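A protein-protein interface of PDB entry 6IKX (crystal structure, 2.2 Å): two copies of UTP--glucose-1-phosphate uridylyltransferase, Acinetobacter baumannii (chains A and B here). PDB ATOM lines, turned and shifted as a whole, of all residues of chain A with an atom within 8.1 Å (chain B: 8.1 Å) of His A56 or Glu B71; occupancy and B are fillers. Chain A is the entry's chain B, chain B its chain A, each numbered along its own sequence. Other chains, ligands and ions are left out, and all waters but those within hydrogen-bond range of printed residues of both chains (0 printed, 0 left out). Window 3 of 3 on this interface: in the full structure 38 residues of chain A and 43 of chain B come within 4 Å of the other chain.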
ATOM      1  N   PRO A   8     -27.588  10.382  -0.344  1.00  0.00           N
ATOM      2  CA  PRO A   8     -26.135  10.203  -0.311  1.00  0.00           C
ATOM      3  C   PRO A   8     -25.539  10.908  -1.538  1.00  0.00           C
ATOM      4  O   PRO A   8     -25.864  10.568  -2.623  1.00  0.00           O
ATOM      5  CB  PRO A   8     -25.965   8.678  -0.208  1.00  0.00           C
ATOM      6  CG  PRO A   8     -27.253   8.080  -0.731  1.00  0.00           C
ATOM      7  CD  PRO A   8     -28.308   9.160  -0.724  1.00  0.00           C
ATOM      8  N   VAL A   9     -24.787  11.974  -1.319  1.00  0.00           N
ATOM      9  CA  VAL A   9     -24.310  12.840  -2.436  1.00  0.00           C
ATOM     10  C   VAL A   9     -22.795  13.101  -2.319  1.00  0.00           C
ATOM     11  O   VAL A   9     -22.304  14.062  -2.924  1.00  0.00           O
ATOM     12  CB  VAL A   9     -25.149  14.139  -2.476  1.00  0.00           C
ATOM     13  CG1 VAL A   9     -26.619  13.834  -2.675  1.00  0.00           C
ATOM     14  CG2 VAL A   9     -24.946  15.013  -1.249  1.00  0.00           C
ATOM     15  N   ALA A  10     -22.061  12.268  -1.591  1.00  0.00           N
ATOM     16  CA  ALA A  10     -20.624  12.448  -1.293  1.00  0.00           C
ATOM     17  C   ALA A  10     -19.741  11.923  -2.428  1.00  0.00           C
ATOM     18  O   ALA A  10     -18.559  12.366  -2.501  1.00  0.00           O
ATOM     19  CB  ALA A  10     -20.272  11.793   0.000  1.00  0.00           C
ATOM     20  N   GLY A  11     -20.301  11.100  -3.317  1.00  0.00           N
ATOM     21  CA  GLY A  11     -19.581  10.535  -4.471  1.00  0.00           C
ATOM     22  C   GLY A  11     -19.124  11.583  -5.462  1.00  0.00           C
ATOM     23  O   GLY A  11     -19.941  12.451  -5.820  1.00  0.00           O
ATOM     24  N   LEU A  12     -17.893  11.450  -5.957  1.00  0.00           N
ATOM     25  CA  LEU A  12     -17.305  12.372  -6.970  1.00  0.00           C
ATOM     26  C   LEU A  12     -17.923  12.148  -8.359  1.00  0.00           C
ATOM     27  O   LEU A  12     -18.029  13.122  -9.119  1.00  0.00           O
ATOM     28  CB  LEU A  12     -15.793  12.200  -6.974  1.00  0.00           C
ATOM     29  CG  LEU A  12     -15.085  12.967  -5.863  1.00  0.00           C
ATOM     30  CD1 LEU A  12     -15.595  12.601  -4.476  1.00  0.00           C
ATOM     31  CD2 LEU A  12     -13.591  12.755  -5.940  1.00  0.00           C
ATOM     32  N   THR A  14     -17.097   9.974 -11.297  1.00  0.00           N
ATOM     33  CA  THR A  14     -16.192   9.804 -12.449  1.00  0.00           C
ATOM     34  C   THR A  14     -16.982   9.295 -13.667  1.00  0.00           C
ATOM     35  O   THR A  14     -16.394   9.225 -14.775  1.00  0.00           O
ATOM     36  CB  THR A  14     -15.029   8.850 -12.114  1.00  0.00           C
ATOM     37  OG1 THR A  14     -15.531   7.516 -11.976  1.00  0.00           O
ATOM     38  CG2 THR A  14     -14.267   9.247 -10.867  1.00  0.00           C
ATOM     39  N   PRO A  24     -20.511  19.623  -8.596  1.00  0.00           N
ATOM     40  CA  PRO A  24     -21.077  18.346  -8.196  1.00  0.00           C
ATOM     41  C   PRO A  24     -21.866  17.810  -9.382  1.00  0.00           C
ATOM     42  O   PRO A  24     -22.445  18.608 -10.071  1.00  0.00           O
ATOM     43  CB  PRO A  24     -21.969  18.750  -7.011  1.00  0.00           C
ATOM     44  CG  PRO A  24     -21.271  19.981  -6.463  1.00  0.00           C
ATOM     45  CD  PRO A  24     -20.962  20.720  -7.732  1.00  0.00           C
ATOM     46  N   GLU A  26     -24.491  16.258  -8.966  1.00  0.00           N
ATOM     47  CA  GLU A  26     -25.892  16.517  -8.542  1.00  0.00           C
ATOM     48  C   GLU A  26     -26.351  17.925  -8.992  1.00  0.00           C
ATOM     49  O   GLU A  26     -27.599  18.147  -9.003  1.00  0.00           O
ATOM     50  CB  GLU A  26     -26.023  16.293  -7.036  1.00  0.00           C
ATOM     51  CG  GLU A  26     -25.644  14.887  -6.608  1.00  0.00           C
ATOM     52  CD  GLU A  26     -24.231  14.713  -6.100  1.00  0.00           C
ATOM     53  OE1 GLU A  26     -23.425  15.659  -6.235  1.00  0.00           O
ATOM     54  OE2 GLU A  26     -23.923  13.614  -5.569  1.00  0.00           O
ATOM     55  N   LEU A  53     -28.601  15.496   3.622  1.00  0.00           N
ATOM     56  CA  LEU A  53     -27.499  15.380   2.631  1.00  0.00           C
ATOM     57  C   LEU A  53     -26.319  14.748   3.349  1.00  0.00           C
ATOM     58  O   LEU A  53     -25.846  15.308   4.355  1.00  0.00           O
ATOM     59  CB  LEU A  53     -27.123  16.742   2.050  1.00  0.00           C
ATOM     60  CG  LEU A  53     -28.264  17.487   1.362  1.00  0.00           C
ATOM     61  CD1 LEU A  53     -27.842  18.891   1.023  1.00  0.00           C
ATOM     62  CD2 LEU A  53     -28.739  16.800   0.101  1.00  0.00           C
ATOM     63  N   VAL A  54     -25.904  13.578   2.864  1.00  0.00           N
ATOM     64  CA  VAL A  54     -24.629  12.938   3.282  1.00  0.00           C
ATOM     65  C   VAL A  54     -23.610  13.317   2.218  1.00  0.00           C
ATOM     66  O   VAL A  54     -23.702  12.784   1.058  1.00  0.00           O
ATOM     67  CB  VAL A  54     -24.764  11.420   3.496  1.00  0.00           C
ATOM     68  CG1 VAL A  54     -23.403  10.807   3.809  1.00  0.00           C
ATOM     69  CG2 VAL A  54     -25.772  11.136   4.620  1.00  0.00           C
ATOM     70  N   THR A  55     -22.786  14.301   2.547  1.00  0.00           N
ATOM     71  CA  THR A  55     -22.123  15.128   1.515  1.00  0.00           C
ATOM     72  C   THR A  55     -20.583  15.094   1.592  1.00  0.00           C
ATOM     73  O   THR A  55     -19.992  14.518   2.562  1.00  0.00           O
ATOM     74  CB  THR A  55     -22.657  16.563   1.632  1.00  0.00           C
ATOM     75  OG1 THR A  55     -22.388  17.201   0.388  1.00  0.00           O
ATOM     76  CG2 THR A  55     -22.022  17.305   2.786  1.00  0.00           C
ATOM     77  N   HIS A  56     -19.963  15.748   0.603  1.00  0.00           N
ATOM     78  CA  HIS A  56     -18.494  15.897   0.466  1.00  0.00           C
ATOM     79  C   HIS A  56     -18.126  17.386   0.537  1.00  0.00           C
ATOM     80  O   HIS A  56     -18.929  18.184   0.035  1.00  0.00           O
ATOM     81  CB  HIS A  56     -18.023  15.210  -0.839  1.00  0.00           C
ATOM     82  CG  HIS A  56     -16.547  15.257  -1.072  1.00  0.00           C
ATOM     83  ND1 HIS A  56     -15.970  16.102  -2.011  1.00  0.00           N
ATOM     84  CD2 HIS A  56     -15.537  14.547  -0.530  1.00  0.00           C
ATOM     85  CE1 HIS A  56     -14.672  15.919  -2.023  1.00  0.00           C
ATOM     86  NE2 HIS A  56     -14.379  14.989  -1.101  1.00  0.00           N
ATOM     87  N   SER A  57     -16.931  17.690   1.060  1.00  0.00           N
ATOM     88  CA  SER A  57     -16.252  19.008   1.131  1.00  0.00           C
ATOM     89  C   SER A  57     -16.334  19.810  -0.188  1.00  0.00           C
ATOM     90  O   SER A  57     -16.169  21.040  -0.143  1.00  0.00           O
ATOM     91  CB  SER A  57     -14.812  18.822   1.551  1.00  0.00           C
ATOM     92  OG  SER A  57     -14.097  18.134   0.545  1.00  0.00           O
ATOM     93  N   SER A  58     -16.571  19.180  -1.323  1.00  0.00           N
ATOM     94  CA  SER A  58     -16.610  19.859  -2.646  1.00  0.00           C
ATOM     95  C   SER A  58     -18.047  20.180  -3.090  1.00  0.00           C
ATOM     96  O   SER A  58     -18.184  20.696  -4.219  1.00  0.00           O
ATOM     97  CB  SER A  58     -15.942  18.997  -3.697  1.00  0.00           C
ATOM     98  OG  SER A  58     -16.733  17.829  -3.908  1.00  0.00           O
ATOM     99  N   LYS A  59     -19.067  19.830  -2.292  1.00  0.00           N
ATOM    100  CA  LYS A  59     -20.514  19.935  -2.648  1.00  0.00           C
ATOM    101  C   LYS A  59     -21.228  21.145  -1.998  1.00  0.00           C
ATOM    102  O   LYS A  59     -22.452  21.134  -1.993  1.00  0.00           O
ATOM    103  CB  LYS A  59     -21.257  18.674  -2.189  1.00  0.00           C
ATOM    104  CG  LYS A  59     -20.768  17.337  -2.726  1.00  0.00           C
ATOM    105  CD  LYS A  59     -20.543  17.280  -4.215  1.00  0.00           C
ATOM    106  CE  LYS A  59     -20.007  15.935  -4.658  1.00  0.00           C
ATOM    107  NZ  LYS A  59     -21.088  14.941  -4.798  1.00  0.00           N
ATOM    108  N   ALA A  60     -20.545  22.179  -1.513  1.00  0.00           N
ATOM    109  CA  ALA A  60     -21.186  23.386  -0.916  1.00  0.00           C
ATOM    110  C   ALA A  60     -22.355  23.861  -1.793  1.00  0.00           C
ATOM    111  O   ALA A  60     -23.452  24.150  -1.253  1.00  0.00           O
ATOM    112  CB  ALA A  60     -20.177  24.492  -0.706  1.00  0.00           C
ATOM    113  N   SER A  61     -22.157  23.898  -3.107  1.00  0.00           N
ATOM    114  CA  SER A  61     -23.148  24.414  -4.075  1.00  0.00           C
ATOM    115  C   SER A  61     -24.490  23.679  -3.953  1.00  0.00           C
ATOM    116  O   SER A  61     -25.526  24.304  -4.308  1.00  0.00           O
ATOM    117  CB  SER A  61     -22.628  24.370  -5.469  1.00  0.00           C
ATOM    118  OG  SER A  61     -22.701  23.073  -5.995  1.00  0.00           O
ATOM    119  N   ILE A  62     -24.495  22.400  -3.557  1.00  0.00           N
ATOM    120  CA  ILE A  62     -25.780  21.676  -3.328  1.00  0.00           C
ATOM    121  C   ILE A  62     -26.519  22.377  -2.174  1.00  0.00           C
ATOM    122  O   ILE A  62     -27.706  22.694  -2.349  1.00  0.00           O
ATOM    123  CB  ILE A  62     -25.580  20.181  -3.020  1.00  0.00           C
ATOM    124  CG1 ILE A  62     -24.974  19.424  -4.203  1.00  0.00           C
ATOM    125  CG2 ILE A  62     -26.903  19.558  -2.587  1.00  0.00           C
ATOM    126  CD1 ILE A  62     -24.638  17.976  -3.876  1.00  0.00           C
ATOM    127  N   GLU A  63     -25.861  22.583  -1.041  1.00  0.00           N
ATOM    128  CA  GLU A  63     -26.500  23.205   0.153  1.00  0.00           C
ATOM    129  C   GLU A  63     -26.944  24.636  -0.190  1.00  0.00           C
ATOM    130  O   GLU A  63     -28.036  25.031   0.218  1.00  0.00           O
ATOM    131  CB  GLU A  63     -25.565  23.205   1.370  1.00  0.00           C
ATOM    132  CG  GLU A  63     -25.371  21.814   1.957  1.00  0.00           C
ATOM    133  CD  GLU A  63     -23.921  21.371   2.109  1.00  0.00           C
ATOM    134  OE1 GLU A  63     -23.230  21.992   2.933  1.00  0.00           O
ATOM    135  OE2 GLU A  63     -23.469  20.420   1.354  1.00  0.00           O
ATOM    136  N   SER A 100     -26.994  18.709   6.650  1.00  0.00           N
ATOM    137  CA  SER A 100     -25.888  18.040   5.968  1.00  0.00           C
ATOM    138  C   SER A 100     -24.941  17.488   7.013  1.00  0.00           C
ATOM    139  O   SER A 100     -24.804  18.087   8.114  1.00  0.00           O
ATOM    140  CB  SER A 100     -25.235  18.959   4.951  1.00  0.00           C
ATOM    141  OG  SER A 100     -24.688  20.067   5.616  1.00  0.00           O
ATOM    142  N   VAL A 101     -24.402  16.321   6.676  1.00  0.00           N
ATOM    143  CA  VAL A 101     -23.361  15.603   7.442  1.00  0.00           C
ATOM    144  C   VAL A 101     -22.340  15.145   6.394  1.00  0.00           C
ATOM    145  O   VAL A 101     -22.763  14.924   5.232  1.00  0.00           O
ATOM    146  CB  VAL A 101     -23.975  14.473   8.307  1.00  0.00           C
ATOM    147  CG1 VAL A 101     -24.703  13.412   7.488  1.00  0.00           C
ATOM    148  CG2 VAL A 101     -22.939  13.842   9.223  1.00  0.00           C
ATOM    149  N   ARG A 102     -21.051  15.194   6.748  1.00  0.00           N
ATOM    150  CA  ARG A 102     -19.943  14.832   5.815  1.00  0.00           C
ATOM    151  C   ARG A 102     -19.751  13.311   5.849  1.00  0.00           C
ATOM    152  O   ARG A 102     -19.691  12.763   6.958  1.00  0.00           O
ATOM    153  CB  ARG A 102     -18.645  15.557   6.192  1.00  0.00           C
ATOM    154  CG  ARG A 102     -18.752  17.056   5.999  1.00  0.00           C
ATOM    155  CD  ARG A 102     -18.937  17.517   4.562  1.00  0.00           C
ATOM    156  NE  ARG A 102     -18.779  18.962   4.510  1.00  0.00           N
ATOM    157  CZ  ARG A 102     -17.609  19.613   4.502  1.00  0.00           C
ATOM    158  NH1 ARG A 102     -16.456  18.970   4.489  1.00  0.00           N
ATOM    159  NH2 ARG A 102     -17.589  20.931   4.471  1.00  0.00           N
ATOM    160  N   GLN A 103     -19.723  12.657   4.691  1.00  0.00           N
ATOM    161  CA  GLN A 103     -19.213  11.272   4.607  1.00  0.00           C
ATOM    162  C   GLN A 103     -17.694  11.400   4.531  1.00  0.00           C
ATOM    163  O   GLN A 103     -17.163  11.673   3.459  1.00  0.00           O
ATOM    164  CB  GLN A 103     -19.804  10.534   3.398  1.00  0.00           C
ATOM    165  CG  GLN A 103     -19.074   9.221   3.118  1.00  0.00           C
ATOM    166  CD  GLN A 103     -19.851   8.241   2.277  1.00  0.00           C
ATOM    167  OE1 GLN A 103     -19.954   7.053   2.603  1.00  0.00           O
ATOM    168  NE2 GLN A 103     -20.400   8.727   1.179  1.00  0.00           N
ATOM    169  N   PRO A 104     -16.949  11.169   5.631  1.00  0.00           N
ATOM    170  CA  PRO A 104     -15.530  11.515   5.668  1.00  0.00           C
ATOM    171  C   PRO A 104     -14.696  10.764   4.610  1.00  0.00           C
ATOM    172  O   PRO A 104     -13.811  11.410   4.062  1.00  0.00           O
ATOM    173  CB  PRO A 104     -15.080  11.148   7.096  1.00  0.00           C
ATOM    174  CG  PRO A 104     -16.168  10.216   7.665  1.00  0.00           C
ATOM    175  CD  PRO A 104     -17.413  10.457   6.840  1.00  0.00           C
ATOM    176  N   GLN A 105     -15.015   9.485   4.295  1.00  0.00           N
ATOM    177  CA  GLN A 105     -14.409   8.737   3.141  1.00  0.00           C
ATOM    178  C   GLN A 105     -15.422   7.973   2.281  1.00  0.00           C
ATOM    179  O   GLN A 105     -16.518   7.670   2.727  1.00  0.00           O
ATOM    180  CB  GLN A 105     -13.346   7.781   3.651  1.00  0.00           C
ATOM    181  CG  GLN A 105     -12.036   8.492   3.871  1.00  0.00           C
ATOM    182  CD  GLN A 105     -11.273   7.782   4.944  1.00  0.00           C
ATOM    183  OE1 GLN A 105     -11.779   6.854   5.566  1.00  0.00           O
ATOM    184  NE2 GLN A 105     -10.047   8.220   5.150  1.00  0.00           N
ATOM    185  N   PRO A 106     -15.081   7.669   1.005  1.00  0.00           N
ATOM    186  CA  PRO A 106     -15.997   7.014   0.078  1.00  0.00           C
ATOM    187  C   PRO A 106     -16.031   5.507   0.323  1.00  0.00           C
ATOM    188  O   PRO A 106     -15.386   4.791  -0.385  1.00  0.00           O
ATOM    189  CB  PRO A 106     -15.457   7.322  -1.339  1.00  0.00           C
ATOM    190  CG  PRO A 106     -14.027   7.767  -1.138  1.00  0.00           C
ATOM    191  CD  PRO A 106     -13.820   8.041   0.345  1.00  0.00           C
ATOM    192  N   ARG B  68      -5.657  21.288 -12.177  1.00  0.00           N
ATOM    193  CA  ARG B  68      -5.649  19.860 -11.788  1.00  0.00           C
ATOM    194  C   ARG B  68      -6.373  19.697 -10.450  1.00  0.00           C
ATOM    195  O   ARG B  68      -6.434  20.631  -9.643  1.00  0.00           O
ATOM    196  CB  ARG B  68      -4.212  19.336 -11.829  1.00  0.00           C
ATOM    197  CG  ARG B  68      -3.832  19.001 -13.263  1.00  0.00           C
ATOM    198  CD  ARG B  68      -2.355  18.897 -13.542  1.00  0.00           C
ATOM    199  NE  ARG B  68      -1.809  17.629 -13.098  1.00  0.00           N
ATOM    200  CZ  ARG B  68      -2.247  16.449 -13.488  1.00  0.00           C
ATOM    201  NH1 ARG B  68      -3.278  16.342 -14.307  1.00  0.00           N
ATOM    202  NH2 ARG B  68      -1.688  15.368 -13.004  1.00  0.00           N
ATOM    203  N   ASN B  69      -6.939  18.524 -10.265  1.00  0.00           N
ATOM    204  CA  ASN B  69      -7.709  18.155  -9.063  1.00  0.00           C
ATOM    205  C   ASN B  69      -7.087  16.868  -8.475  1.00  0.00           C
ATOM    206  O   ASN B  69      -7.231  15.792  -9.065  1.00  0.00           O
ATOM    207  CB  ASN B  69      -9.183  18.072  -9.461  1.00  0.00           C
ATOM    208  CG  ASN B  69     -10.054  17.564  -8.341  1.00  0.00           C
ATOM    209  OD1 ASN B  69     -11.272  17.583  -8.468  1.00  0.00           O
ATOM    210  ND2 ASN B  69      -9.443  17.118  -7.250  1.00  0.00           N
ATOM    211  N   PHE B  70      -6.427  16.972  -7.334  1.00  0.00           N
ATOM    212  CA  PHE B  70      -5.682  15.841  -6.726  1.00  0.00           C
ATOM    213  C   PHE B  70      -6.623  14.662  -6.457  1.00  0.00           C
ATOM    214  O   PHE B  70      -6.443  13.633  -7.089  1.00  0.00           O
ATOM    215  CB  PHE B  70      -4.948  16.287  -5.472  1.00  0.00           C
ATOM    216  CG  PHE B  70      -3.989  15.245  -4.972  1.00  0.00           C
ATOM    217  CD1 PHE B  70      -2.789  15.021  -5.632  1.00  0.00           C
ATOM    218  CD2 PHE B  70      -4.329  14.426  -3.901  1.00  0.00           C
ATOM    219  CE1 PHE B  70      -1.915  14.043  -5.188  1.00  0.00           C
ATOM    220  CE2 PHE B  70      -3.443  13.467  -3.451  1.00  0.00           C
ATOM    221  CZ  PHE B  70      -2.242  13.276  -4.099  1.00  0.00           C
ATOM    222  N   GLU B  71      -7.656  14.862  -5.643  1.00  0.00           N
ATOM    223  CA  GLU B  71      -8.618  13.809  -5.231  1.00  0.00           C
ATOM    224  C   GLU B  71      -9.301  13.221  -6.461  1.00  0.00           C
ATOM    225  O   GLU B  71      -9.649  12.047  -6.429  1.00  0.00           O
ATOM    226  CB  GLU B  71      -9.664  14.345  -4.254  1.00  0.00           C
ATOM    227  CG  GLU B  71     -10.496  13.267  -3.591  1.00  0.00           C
ATOM    228  CD  GLU B  71     -11.314  13.718  -2.382  1.00  0.00           C
ATOM    229  OE1 GLU B  71     -11.193  14.907  -1.978  1.00  0.00           O
ATOM    230  OE2 GLU B  71     -12.054  12.869  -1.816  1.00  0.00           O
ATOM    231  N   LEU B  72      -9.573  14.000  -7.496  1.00  0.00           N
ATOM    232  CA  LEU B  72     -10.384  13.441  -8.604  1.00  0.00           C
ATOM    233  C   LEU B  72      -9.528  12.422  -9.367  1.00  0.00           C
ATOM    234  O   LEU B  72     -10.025  11.348  -9.722  1.00  0.00           O
ATOM    235  CB  LEU B  72     -10.852  14.553  -9.531  1.00  0.00           C
ATOM    236  CG  LEU B  72     -11.636  14.036 -10.733  1.00  0.00           C
ATOM    237  CD1 LEU B  72     -12.827  13.196 -10.250  1.00  0.00           C
ATOM    238  CD2 LEU B  72     -12.075  15.174 -11.642  1.00  0.00           C
ATOM    239  N   GLU B  73      -8.282  12.800  -9.614  1.00  0.00           N
ATOM    240  CA  GLU B  73      -7.286  12.043 -10.403  1.00  0.00           C
ATOM    241  C   GLU B  73      -6.979  10.730  -9.674  1.00  0.00           C
ATOM    242  O   GLU B  73      -7.101   9.680 -10.316  1.00  0.00           O
ATOM    243  CB  GLU B  73      -6.068  12.941 -10.648  1.00  0.00           C
ATOM    244  CG  GLU B  73      -6.350  13.966 -11.728  1.00  0.00           C
ATOM    245  CD  GLU B  73      -5.366  15.109 -11.829  1.00  0.00           C
ATOM    246  OE1 GLU B  73      -4.203  14.948 -11.402  1.00  0.00           O
ATOM    247  OE2 GLU B  73      -5.765  16.157 -12.342  1.00  0.00           O
ATOM    248  N   THR B  74      -6.712  10.772  -8.371  1.00  0.00           N
ATOM    249  CA  THR B  74      -6.359   9.548  -7.636  1.00  0.00           C
ATOM    250  C   THR B  74      -7.591   8.642  -7.579  1.00  0.00           C
ATOM    251  O   THR B  74      -7.405   7.448  -7.769  1.00  0.00           O
ATOM    252  CB  THR B  74      -5.608   9.788  -6.323  1.00  0.00           C
ATOM    253  OG1 THR B  74      -6.358   9.034  -5.381  1.00  0.00           O
ATOM    254  CG2 THR B  74      -5.404  11.228  -5.914  1.00  0.00           C
ATOM    255  N   THR B  75      -8.805   9.165  -7.482  1.00  0.00           N
ATOM    256  CA  THR B  75     -10.020   8.328  -7.627  1.00  0.00           C
ATOM    257  C   THR B  75      -9.967   7.638  -8.992  1.00  0.00           C
ATOM    258  O   THR B  75     -10.211   6.433  -9.012  1.00  0.00           O
ATOM    259  CB  THR B  75     -11.319   9.126  -7.497  1.00  0.00           C
ATOM    260  OG1 THR B  75     -11.336   9.822  -6.251  1.00  0.00           O
ATOM    261  CG2 THR B  75     -12.551   8.252  -7.599  1.00  0.00           C
ATOM    262  N   LEU B  76      -9.657   8.380 -10.067  1.00  0.00           N
ATOM    263  CA  LEU B  76      -9.648   7.888 -11.479  1.00  0.00           C
ATOM    264  C   LEU B  76      -8.547   6.836 -11.692  1.00  0.00           C
ATOM    265  O   LEU B  76      -8.771   5.922 -12.520  1.00  0.00           O
ATOM    266  CB  LEU B  76      -9.430   9.043 -12.464  1.00  0.00           C
ATOM    267  CG  LEU B  76     -10.630   9.919 -12.807  1.00  0.00           C
ATOM    268  CD1 LEU B  76     -10.227  11.006 -13.794  1.00  0.00           C
ATOM    269  CD2 LEU B  76     -11.750   9.113 -13.408  1.00  0.00           C
ATOM    270  N   GLU B  77      -7.380   7.007 -11.064  1.00  0.00           N
ATOM    271  CA  GLU B  77      -6.274   6.006 -11.090  1.00  0.00           C
ATOM    272  C   GLU B  77      -6.704   4.719 -10.372  1.00  0.00           C
ATOM    273  O   GLU B  77      -6.745   3.670 -11.012  1.00  0.00           O
ATOM    274  CB  GLU B  77      -5.035   6.532 -10.383  1.00  0.00           C
ATOM    275  CG  GLU B  77      -3.948   7.015 -11.307  1.00  0.00           C
ATOM    276  CD  GLU B  77      -3.061   8.014 -10.599  1.00  0.00           C
ATOM    277  OE1 GLU B  77      -2.732   7.764  -9.411  1.00  0.00           O
ATOM    278  OE2 GLU B  77      -2.773   9.069 -11.202  1.00  0.00           O
ATOM    279  N   GLN B  78      -7.055   4.817  -9.094  1.00  0.00           N
ATOM    280  CA  GLN B  78      -7.546   3.686  -8.264  1.00  0.00           C
ATOM    281  C   GLN B  78      -8.583   2.840  -9.011  1.00  0.00           C
ATOM    282  O   GLN B  78      -8.600   1.623  -8.744  1.00  0.00           O
ATOM    283  CB  GLN B  78      -8.104   4.198  -6.939  1.00  0.00           C
ATOM    284  CG  GLN B  78      -6.994   4.678  -6.007  1.00  0.00           C
ATOM    285  CD  GLN B  78      -7.510   5.354  -4.759  1.00  0.00           C
ATOM    286  OE1 GLN B  78      -8.690   5.654  -4.643  1.00  0.00           O
ATOM    287  NE2 GLN B  78      -6.617   5.621  -3.820  1.00  0.00           N
ATOM    288  N   ILE B  88      -9.136  14.546 -18.732  1.00  0.00           N
ATOM    289  CA  ILE B  88      -9.471  15.614 -17.733  1.00  0.00           C
ATOM    290  C   ILE B  88      -8.183  16.273 -17.215  1.00  0.00           C
ATOM    291  O   ILE B  88      -8.275  17.272 -16.479  1.00  0.00           O
ATOM    292  CB  ILE B  88     -10.394  15.072 -16.608  1.00  0.00           C
ATOM    293  CG1 ILE B  88      -9.707  14.067 -15.692  1.00  0.00           C
ATOM    294  CG2 ILE B  88     -11.680  14.507 -17.198  1.00  0.00           C
ATOM    295  CD1 ILE B  88      -9.425  14.579 -14.295  1.00  0.00           C
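The backbone NH (N) of Glu B71 lies close to the side-chain amide nitrogen (ND2) of Asn B69 (3.3 Å). OG1 of Thr B75 lies within hydrogen-bond range of O of Glu B71, at 2.8 Å. ND1 of His A56 lies within hydrogen-bond range of OG of Ser A58 (2.7 Å).
A ring nitrogen (NE2) of His A56 is in hydrogen-bond range of the side-chain carboxylate (OE2) of Glu B71 (3.2 Å).
CD2 of Leu A12 touches CG of Glu B71, 3.9 Å away. Leu A12 touches Thr B75. CG2 of Thr B75 touches CG2 of Thr A14, 3.8 Å away. CD2 of Leu B76 touches CB of Thr A14, 3.5 Å away.
Of chain A, only Leu A12 and His A56 come within 4 Å of Glu B71. No residue of chain B comes within 4 Å of Thr A55. No residue of chain B comes within 4 Å of Ser A57. Of the printed residues of chain B, Thr A14 touches Thr B75 and Leu B76. Printed residues of chain A within 4 Å of Thr B75: Leu A12 and Thr A14. Of the printed residues of chain A, Leu B76 touches Thr A14 (3.5 Å). Ala A10 touches none of the printed residues of chain B. Arg B68 touches none of the printed residues of chain A. The nearest residue of chain B that does not touch His A56 is Asn B69 (7.5 Å). The nearest residue of chain A that does not touch Glu B71 is Ser A57 (5.0 Å). The nearest printed residue of chain A that does not touch Thr B75 is Pro A106 (6.1 Å).
Hydrophobic or aromatic side chains of chain A within 4 Å of the printed part of chain B: Leu A12 and His A56. Hydrophobic or aromatic side chains of chain B within 4 Å of the printed part of chain A: Leu B76. Among the printed residues, 5 pairs touch across the chains.
No position is printed for both chains. Of the 5 pairs that touch across the chains among the printed residues, none has its exchanged pair printed and touching as well.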
